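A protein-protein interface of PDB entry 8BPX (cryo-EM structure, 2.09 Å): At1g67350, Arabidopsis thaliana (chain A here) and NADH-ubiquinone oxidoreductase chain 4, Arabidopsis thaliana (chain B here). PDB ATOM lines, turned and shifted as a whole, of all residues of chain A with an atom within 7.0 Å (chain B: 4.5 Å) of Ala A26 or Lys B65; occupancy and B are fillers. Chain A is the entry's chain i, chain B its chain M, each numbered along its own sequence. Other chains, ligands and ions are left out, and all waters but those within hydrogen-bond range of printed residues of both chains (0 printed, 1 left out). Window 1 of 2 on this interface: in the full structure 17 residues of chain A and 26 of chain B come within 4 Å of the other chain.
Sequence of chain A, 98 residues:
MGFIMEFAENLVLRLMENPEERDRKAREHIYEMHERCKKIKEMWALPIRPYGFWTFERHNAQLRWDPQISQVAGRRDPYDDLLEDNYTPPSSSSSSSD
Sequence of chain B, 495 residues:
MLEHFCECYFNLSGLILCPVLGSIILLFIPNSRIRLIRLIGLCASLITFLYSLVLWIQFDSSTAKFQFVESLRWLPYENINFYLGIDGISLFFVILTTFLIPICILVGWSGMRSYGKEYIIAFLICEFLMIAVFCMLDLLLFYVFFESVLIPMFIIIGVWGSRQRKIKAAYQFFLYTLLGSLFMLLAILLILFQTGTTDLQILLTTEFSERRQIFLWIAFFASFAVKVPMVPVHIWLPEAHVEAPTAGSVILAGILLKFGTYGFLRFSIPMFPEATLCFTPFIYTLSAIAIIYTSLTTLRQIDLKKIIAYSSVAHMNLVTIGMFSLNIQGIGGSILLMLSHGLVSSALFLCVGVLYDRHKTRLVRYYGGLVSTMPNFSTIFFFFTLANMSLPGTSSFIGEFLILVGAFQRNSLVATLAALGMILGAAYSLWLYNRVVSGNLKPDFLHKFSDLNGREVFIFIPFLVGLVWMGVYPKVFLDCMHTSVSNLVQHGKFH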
ATOM      1  N   PRO A  19     -16.545 -28.235   0.921  1.00  0.00           N
ATOM      2  CA  PRO A  19     -17.312 -27.101   1.486  1.00  0.00           C
ATOM      3  C   PRO A  19     -18.772 -27.415   1.804  1.00  0.00           C
ATOM      4  O   PRO A  19     -19.271 -26.916   2.773  1.00  0.00           O
ATOM      5  CB  PRO A  19     -17.212 -26.033   0.377  1.00  0.00           C
ATOM      6  CG  PRO A  19     -16.893 -26.799  -0.880  1.00  0.00           C
ATOM      7  CD  PRO A  19     -16.042 -27.960  -0.424  1.00  0.00           C
ATOM      8  N   GLU A  21     -20.070 -30.484   2.701  1.00  0.00           N
ATOM      9  CA  GLU A  21     -20.154 -31.279   3.922  1.00  0.00           C
ATOM     10  C   GLU A  21     -19.781 -30.458   5.151  1.00  0.00           C
ATOM     11  O   GLU A  21     -20.376 -30.628   6.220  1.00  0.00           O
ATOM     12  CB  GLU A  21     -19.263 -32.516   3.810  1.00  0.00           C
ATOM     13  CG  GLU A  21     -19.741 -33.536   2.788  1.00  0.00           C
ATOM     14  CD  GLU A  21     -18.666 -34.539   2.417  1.00  0.00           C
ATOM     15  OE1 GLU A  21     -17.706 -34.700   3.201  1.00  0.00           O
ATOM     16  OE2 GLU A  21     -18.781 -35.168   1.344  1.00  0.00           O
ATOM     17  N   ARG A  22     -18.786 -29.579   5.011  1.00  0.00           N
ATOM     18  CA  ARG A  22     -18.355 -28.738   6.160  1.00  0.00           C
ATOM     19  C   ARG A  22     -19.537 -27.846   6.589  1.00  0.00           C
ATOM     20  O   ARG A  22     -19.865 -27.861   7.784  1.00  0.00           O
ATOM     21  CB  ARG A  22     -17.066 -27.969   5.865  1.00  0.00           C
ATOM     22  CG  ARG A  22     -16.653 -27.030   6.987  1.00  0.00           C
ATOM     23  CD  ARG A  22     -16.644 -25.584   6.555  1.00  0.00           C
ATOM     24  NE  ARG A  22     -15.683 -25.434   5.480  1.00  0.00           N
ATOM     25  CZ  ARG A  22     -15.925 -24.839   4.324  1.00  0.00           C
ATOM     26  NH1 ARG A  22     -17.110 -24.307   4.083  1.00  0.00           N
ATOM     27  NH2 ARG A  22     -14.976 -24.778   3.414  1.00  0.00           N
ATOM     28  N   ASP A  23     -20.193 -27.164   5.643  1.00  0.00           N
ATOM     29  CA  ASP A  23     -21.329 -26.314   5.988  1.00  0.00           C
ATOM     30  C   ASP A  23     -22.505 -27.133   6.502  1.00  0.00           C
ATOM     31  O   ASP A  23     -23.234 -26.680   7.394  1.00  0.00           O
ATOM     32  CB  ASP A  23     -21.742 -25.477   4.781  1.00  0.00           C
ATOM     33  CG  ASP A  23     -20.734 -24.392   4.455  1.00  0.00           C
ATOM     34  OD1 ASP A  23     -19.906 -24.071   5.330  1.00  0.00           O
ATOM     35  OD2 ASP A  23     -20.770 -23.861   3.325  1.00  0.00           O
ATOM     36  N   ARG A  24     -22.766 -28.438   6.173  1.00  0.00           N
ATOM     37  CA  ARG A  24     -23.872 -29.361   6.686  1.00  0.00           C
ATOM     38  C   ARG A  24     -23.744 -29.968   8.140  1.00  0.00           C
ATOM     39  O   ARG A  24     -24.745 -29.998   8.879  1.00  0.00           O
ATOM     40  CB  ARG A  24     -24.120 -30.634   5.869  1.00  0.00           C
ATOM     41  CG  ARG A  24     -25.377 -31.371   6.302  1.00  0.00           C
ATOM     42  CD  ARG A  24     -25.680 -32.749   5.761  1.00  0.00           C
ATOM     43  NE  ARG A  24     -24.589 -33.696   5.780  1.00  0.00           N
ATOM     44  CZ  ARG A  24     -24.073 -34.235   6.870  1.00  0.00           C
ATOM     45  NH1 ARG A  24     -24.537 -33.907   8.063  1.00  0.00           N
ATOM     46  NH2 ARG A  24     -23.072 -35.083   6.760  1.00  0.00           N
ATOM     47  N   LYS A  25     -22.588 -30.503   8.535  1.00  0.00           N
ATOM     48  CA  LYS A  25     -22.369 -30.850   9.970  1.00  0.00           C
ATOM     49  C   LYS A  25     -22.533 -29.582  10.842  1.00  0.00           C
ATOM     50  O   LYS A  25     -23.019 -29.700  11.942  1.00  0.00           O
ATOM     51  CB  LYS A  25     -21.016 -31.533  10.133  1.00  0.00           C
ATOM     52  CG  LYS A  25     -20.841 -32.905   9.521  1.00  0.00           C
ATOM     53  CD  LYS A  25     -19.415 -33.357   9.668  1.00  0.00           C
ATOM     54  CE  LYS A  25     -18.449 -32.605   8.781  1.00  0.00           C
ATOM     55  NZ  LYS A  25     -17.085 -32.568   9.354  1.00  0.00           N
ATOM     56  N   ALA A  26     -22.206 -28.402  10.335  1.00  0.00           N
ATOM     57  CA  ALA A  26     -22.381 -27.112  11.035  1.00  0.00           C
ATOM     58  C   ALA A  26     -23.876 -26.893  11.370  1.00  0.00           C
ATOM     59  O   ALA A  26     -24.188 -26.478  12.498  1.00  0.00           O
ATOM     60  CB  ALA A  26     -21.769 -25.987  10.249  1.00  0.00           C
ATOM     61  N   ARG A  27     -24.765 -27.252  10.477  1.00  0.00           N
ATOM     62  CA  ARG A  27     -26.221 -27.119  10.710  1.00  0.00           C
ATOM     63  C   ARG A  27     -26.719 -28.166  11.737  1.00  0.00           C
ATOM     64  O   ARG A  27     -27.442 -27.817  12.615  1.00  0.00           O
ATOM     65  CB  ARG A  27     -26.951 -27.096   9.373  1.00  0.00           C
ATOM     66  CG  ARG A  27     -26.660 -25.853   8.540  1.00  0.00           C
ATOM     67  CD  ARG A  27     -27.591 -25.637   7.363  1.00  0.00           C
ATOM     68  NE  ARG A  27     -27.617 -26.850   6.567  1.00  0.00           N
ATOM     69  CZ  ARG A  27     -26.826 -27.105   5.537  1.00  0.00           C
ATOM     70  NH1 ARG A  27     -25.944 -26.211   5.123  1.00  0.00           N
ATOM     71  NH2 ARG A  27     -26.926 -28.265   4.924  1.00  0.00           N
ATOM     72  N   GLU A  28     -26.203 -29.375  11.653  1.00  0.00           N
ATOM     73  CA  GLU A  28     -26.640 -30.452  12.578  1.00  0.00           C
ATOM     74  C   GLU A  28     -26.256 -30.094  14.030  1.00  0.00           C
ATOM     75  O   GLU A  28     -27.113 -30.172  14.847  1.00  0.00           O
ATOM     76  CB  GLU A  28     -26.181 -31.771  12.020  1.00  0.00           C
ATOM     77  CG  GLU A  28     -26.678 -32.956  12.826  1.00  0.00           C
ATOM     78  CD  GLU A  28     -26.402 -34.320  12.218  1.00  0.00           C
ATOM     79  OE1 GLU A  28     -25.634 -34.389  11.242  1.00  0.00           O
ATOM     80  OE2 GLU A  28     -26.960 -35.309  12.725  1.00  0.00           O
ATOM     81  N   HIS A  29     -25.080 -29.526  14.250  1.00  0.00           N
ATOM     82  CA  HIS A  29     -24.609 -29.112  15.590  1.00  0.00           C
ATOM     83  C   HIS A  29     -25.581 -28.121  16.223  1.00  0.00           C
ATOM     84  O   HIS A  29     -26.051 -28.434  17.233  1.00  0.00           O
ATOM     85  CB  HIS A  29     -23.152 -28.647  15.476  1.00  0.00           C
ATOM     86  CG  HIS A  29     -22.641 -27.887  16.648  1.00  0.00           C
ATOM     87  ND1 HIS A  29     -21.815 -28.447  17.579  1.00  0.00           N
ATOM     88  CD2 HIS A  29     -22.825 -26.609  17.033  1.00  0.00           C
ATOM     89  CE1 HIS A  29     -21.507 -27.557  18.485  1.00  0.00           C
ATOM     90  NE2 HIS A  29     -22.119 -26.426  18.177  1.00  0.00           N
ATOM     91  N   ILE A  30     -25.898 -27.040  15.554  1.00  0.00           N
ATOM     92  CA  ILE A  30     -26.867 -26.028  16.023  1.00  0.00           C
ATOM     93  C   ILE A  30     -28.273 -26.586  16.187  1.00  0.00           C
ATOM     94  O   ILE A  30     -28.867 -26.313  17.185  1.00  0.00           O
ATOM     95  CB  ILE A  30     -26.880 -24.819  15.055  1.00  0.00           C
ATOM     96  CG1 ILE A  30     -25.570 -24.036  15.101  1.00  0.00           C
ATOM     97  CG2 ILE A  30     -28.072 -23.917  15.320  1.00  0.00           C
ATOM     98  CD1 ILE A  30     -25.314 -23.248  13.836  1.00  0.00           C
ATOM     99  N   TYR A  31     -28.765 -27.325  15.204  1.00  0.00           N
ATOM    100  CA  TYR A  31     -30.171 -27.763  15.267  1.00  0.00           C
ATOM    101  C   TYR A  31     -30.215 -28.731  16.428  1.00  0.00           C
ATOM    102  O   TYR A  31     -31.062 -28.622  17.287  1.00  0.00           O
ATOM    103  CB  TYR A  31     -30.648 -28.403  13.968  1.00  0.00           C
ATOM    104  CG  TYR A  31     -32.033 -28.976  13.986  1.00  0.00           C
ATOM    105  CD1 TYR A  31     -33.139 -28.157  14.068  1.00  0.00           C
ATOM    106  CD2 TYR A  31     -32.234 -30.334  13.864  1.00  0.00           C
ATOM    107  CE1 TYR A  31     -34.421 -28.677  14.045  1.00  0.00           C
ATOM    108  CE2 TYR A  31     -33.508 -30.871  13.831  1.00  0.00           C
ATOM    109  CZ  TYR A  31     -34.605 -30.041  13.934  1.00  0.00           C
ATOM    110  OH  TYR A  31     -35.864 -30.568  13.928  1.00  0.00           O
ATOM    111  N   HIS B   4     -17.690 -34.212  14.985  1.00  0.00           N
ATOM    112  CA  HIS B   4     -17.450 -33.243  13.924  1.00  0.00           C
ATOM    113  C   HIS B   4     -16.103 -33.464  13.246  1.00  0.00           C
ATOM    114  O   HIS B   4     -15.459 -32.501  12.816  1.00  0.00           O
ATOM    115  CB  HIS B   4     -17.542 -31.829  14.500  1.00  0.00           C
ATOM    116  CG  HIS B   4     -18.039 -30.800  13.534  1.00  0.00           C
ATOM    117  ND1 HIS B   4     -18.912 -29.801  13.905  1.00  0.00           N
ATOM    118  CD2 HIS B   4     -17.762 -30.592  12.225  1.00  0.00           C
ATOM    119  CE1 HIS B   4     -19.165 -29.033  12.861  1.00  0.00           C
ATOM    120  NE2 HIS B   4     -18.477 -29.489  11.831  1.00  0.00           N
ATOM    121  N   THR B  63     -15.554 -18.648   3.087  1.00  0.00           N
ATOM    122  CA  THR B  63     -16.614 -18.962   4.028  1.00  0.00           C
ATOM    123  C   THR B  63     -16.513 -18.088   5.271  1.00  0.00           C
ATOM    124  O   THR B  63     -15.427 -17.666   5.674  1.00  0.00           O
ATOM    125  CB  THR B  63     -16.558 -20.435   4.431  1.00  0.00           C
ATOM    126  OG1 THR B  63     -17.420 -20.657   5.549  1.00  0.00           O
ATOM    127  CG2 THR B  63     -15.143 -20.819   4.823  1.00  0.00           C
ATOM    128  N   ALA B  64     -17.666 -17.808   5.870  1.00  0.00           N
ATOM    129  CA  ALA B  64     -17.709 -17.182   7.181  1.00  0.00           C
ATOM    130  C   ALA B  64     -17.698 -18.200   8.312  1.00  0.00           C
ATOM    131  O   ALA B  64     -17.607 -17.806   9.479  1.00  0.00           O
ATOM    132  CB  ALA B  64     -18.949 -16.289   7.303  1.00  0.00           C
ATOM    133  N   LYS B  65     -17.777 -19.489   7.994  1.00  0.00           N
ATOM    134  CA  LYS B  65     -17.824 -20.529   9.007  1.00  0.00           C
ATOM    135  C   LYS B  65     -16.438 -20.754   9.612  1.00  0.00           C
ATOM    136  O   LYS B  65     -15.445 -20.123   9.234  1.00  0.00           O
ATOM    137  CB  LYS B  65     -18.352 -21.831   8.407  1.00  0.00           C
ATOM    138  CG  LYS B  65     -19.661 -21.705   7.648  1.00  0.00           C
ATOM    139  CD  LYS B  65     -20.782 -21.179   8.521  1.00  0.00           C
ATOM    140  CE  LYS B  65     -22.129 -21.675   8.015  1.00  0.00           C
ATOM    141  NZ  LYS B  65     -22.073 -23.126   7.678  1.00  0.00           N
ATOM    142  N   PHE B  66     -16.381 -21.675  10.569  1.00  0.00           N
ATOM    143  CA  PHE B  66     -15.125 -22.135  11.142  1.00  0.00           C
ATOM    144  C   PHE B  66     -14.620 -23.314  10.322  1.00  0.00           C
ATOM    145  O   PHE B  66     -15.384 -24.233  10.012  1.00  0.00           O
ATOM    146  CB  PHE B  66     -15.315 -22.545  12.604  1.00  0.00           C
ATOM    147  CG  PHE B  66     -15.591 -21.395  13.528  1.00  0.00           C
ATOM    148  CD1 PHE B  66     -14.728 -20.316  13.596  1.00  0.00           C
ATOM    149  CD2 PHE B  66     -16.723 -21.389  14.321  1.00  0.00           C
ATOM    150  CE1 PHE B  66     -14.990 -19.258  14.449  1.00  0.00           C
ATOM    151  CE2 PHE B  66     -16.988 -20.336  15.167  1.00  0.00           C
ATOM    152  CZ  PHE B  66     -16.119 -19.268  15.230  1.00  0.00           C
ATOM    153  N   GLN B  67     -13.312 -23.485  10.284  1.00  0.00           N
ATOM    154  CA  GLN B  67     -12.755 -24.526   9.391  1.00  0.00           C
ATOM    155  C   GLN B  67     -11.949 -25.572  10.163  1.00  0.00           C
ATOM    156  O   GLN B  67     -11.560 -25.299  11.299  1.00  0.00           O
ATOM    157  CB  GLN B  67     -11.914 -23.849   8.306  1.00  0.00           C
ATOM    158  CG  GLN B  67     -12.686 -22.880   7.435  1.00  0.00           C
ATOM    159  CD  GLN B  67     -11.767 -22.140   6.499  1.00  0.00           C
ATOM    160  OE1 GLN B  67     -10.934 -22.728   5.816  1.00  0.00           O
ATOM    161  NE2 GLN B  67     -11.927 -20.834   6.449  1.00  0.00           N
ATOM    162  N   ASP B  87     -10.482 -19.634  11.911  1.00  0.00           N
ATOM    163  CA  ASP B  87     -11.082 -18.835  10.853  1.00  0.00           C
ATOM    164  C   ASP B  87     -10.006 -17.882  10.347  1.00  0.00           C
ATOM    165  O   ASP B  87      -8.814 -18.079  10.609  1.00  0.00           O
ATOM    166  CB  ASP B  87     -12.344 -18.118  11.360  1.00  0.00           C
ATOM    167  CG  ASP B  87     -12.084 -17.278  12.594  1.00  0.00           C
ATOM    168  OD1 ASP B  87     -11.174 -16.430  12.560  1.00  0.00           O
ATOM    169  OD2 ASP B  87     -12.795 -17.461  13.601  1.00  0.00           O
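OD1 of Asp A23 is in salt-bridge range of NZ of Lys B65 (3.3 Å).
The backbone NH (N) of Lys B65 lies within hydrogen-bond range of the side-chain hydroxyl (OG1) of Thr B63 (2.7 Å). NH1 of Arg A22 lies within salt-bridge range of OD1 of Asp A23 (3.1 Å).
Among the printed residues, pairs that only touch across the chains: Arg A22 with Thr B63, Arg A22 with Phe B66, Lys A25 with His B4 and Ala A26 with Lys B65.
Printed residues of chain B within 4 Å of Arg A22: Thr B63 (3.9 Å) and Phe B66 (3.9 Å). Of the printed residues of chain B, Asp A23 touches Lys B65 (3.3 Å). Printed residues of chain B within 4 Å of Lys A25: His B4. Printed residues of chain B within 4 Å of Ala A26: Lys B65. Printed residues of chain A within 4 Å of His B4: Lys A25. Of chain A, only Asp A23 and Ala A26 come within 4 Å of Lys B65. The nearest printed residue of chain B that does not touch Ala A26 is His B4 (4.003 Å). The nearest printed residue of chain B that does not touch Asp A23 is Thr B63 (4.2 Å).
Of the 7 printed residues of chain B, 4 touch a printed residue of chain A. Of the 12 printed residues of chain A, 4 touch a printed residue of chain B. Among the printed residues, 5 pairs touch across the chains.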
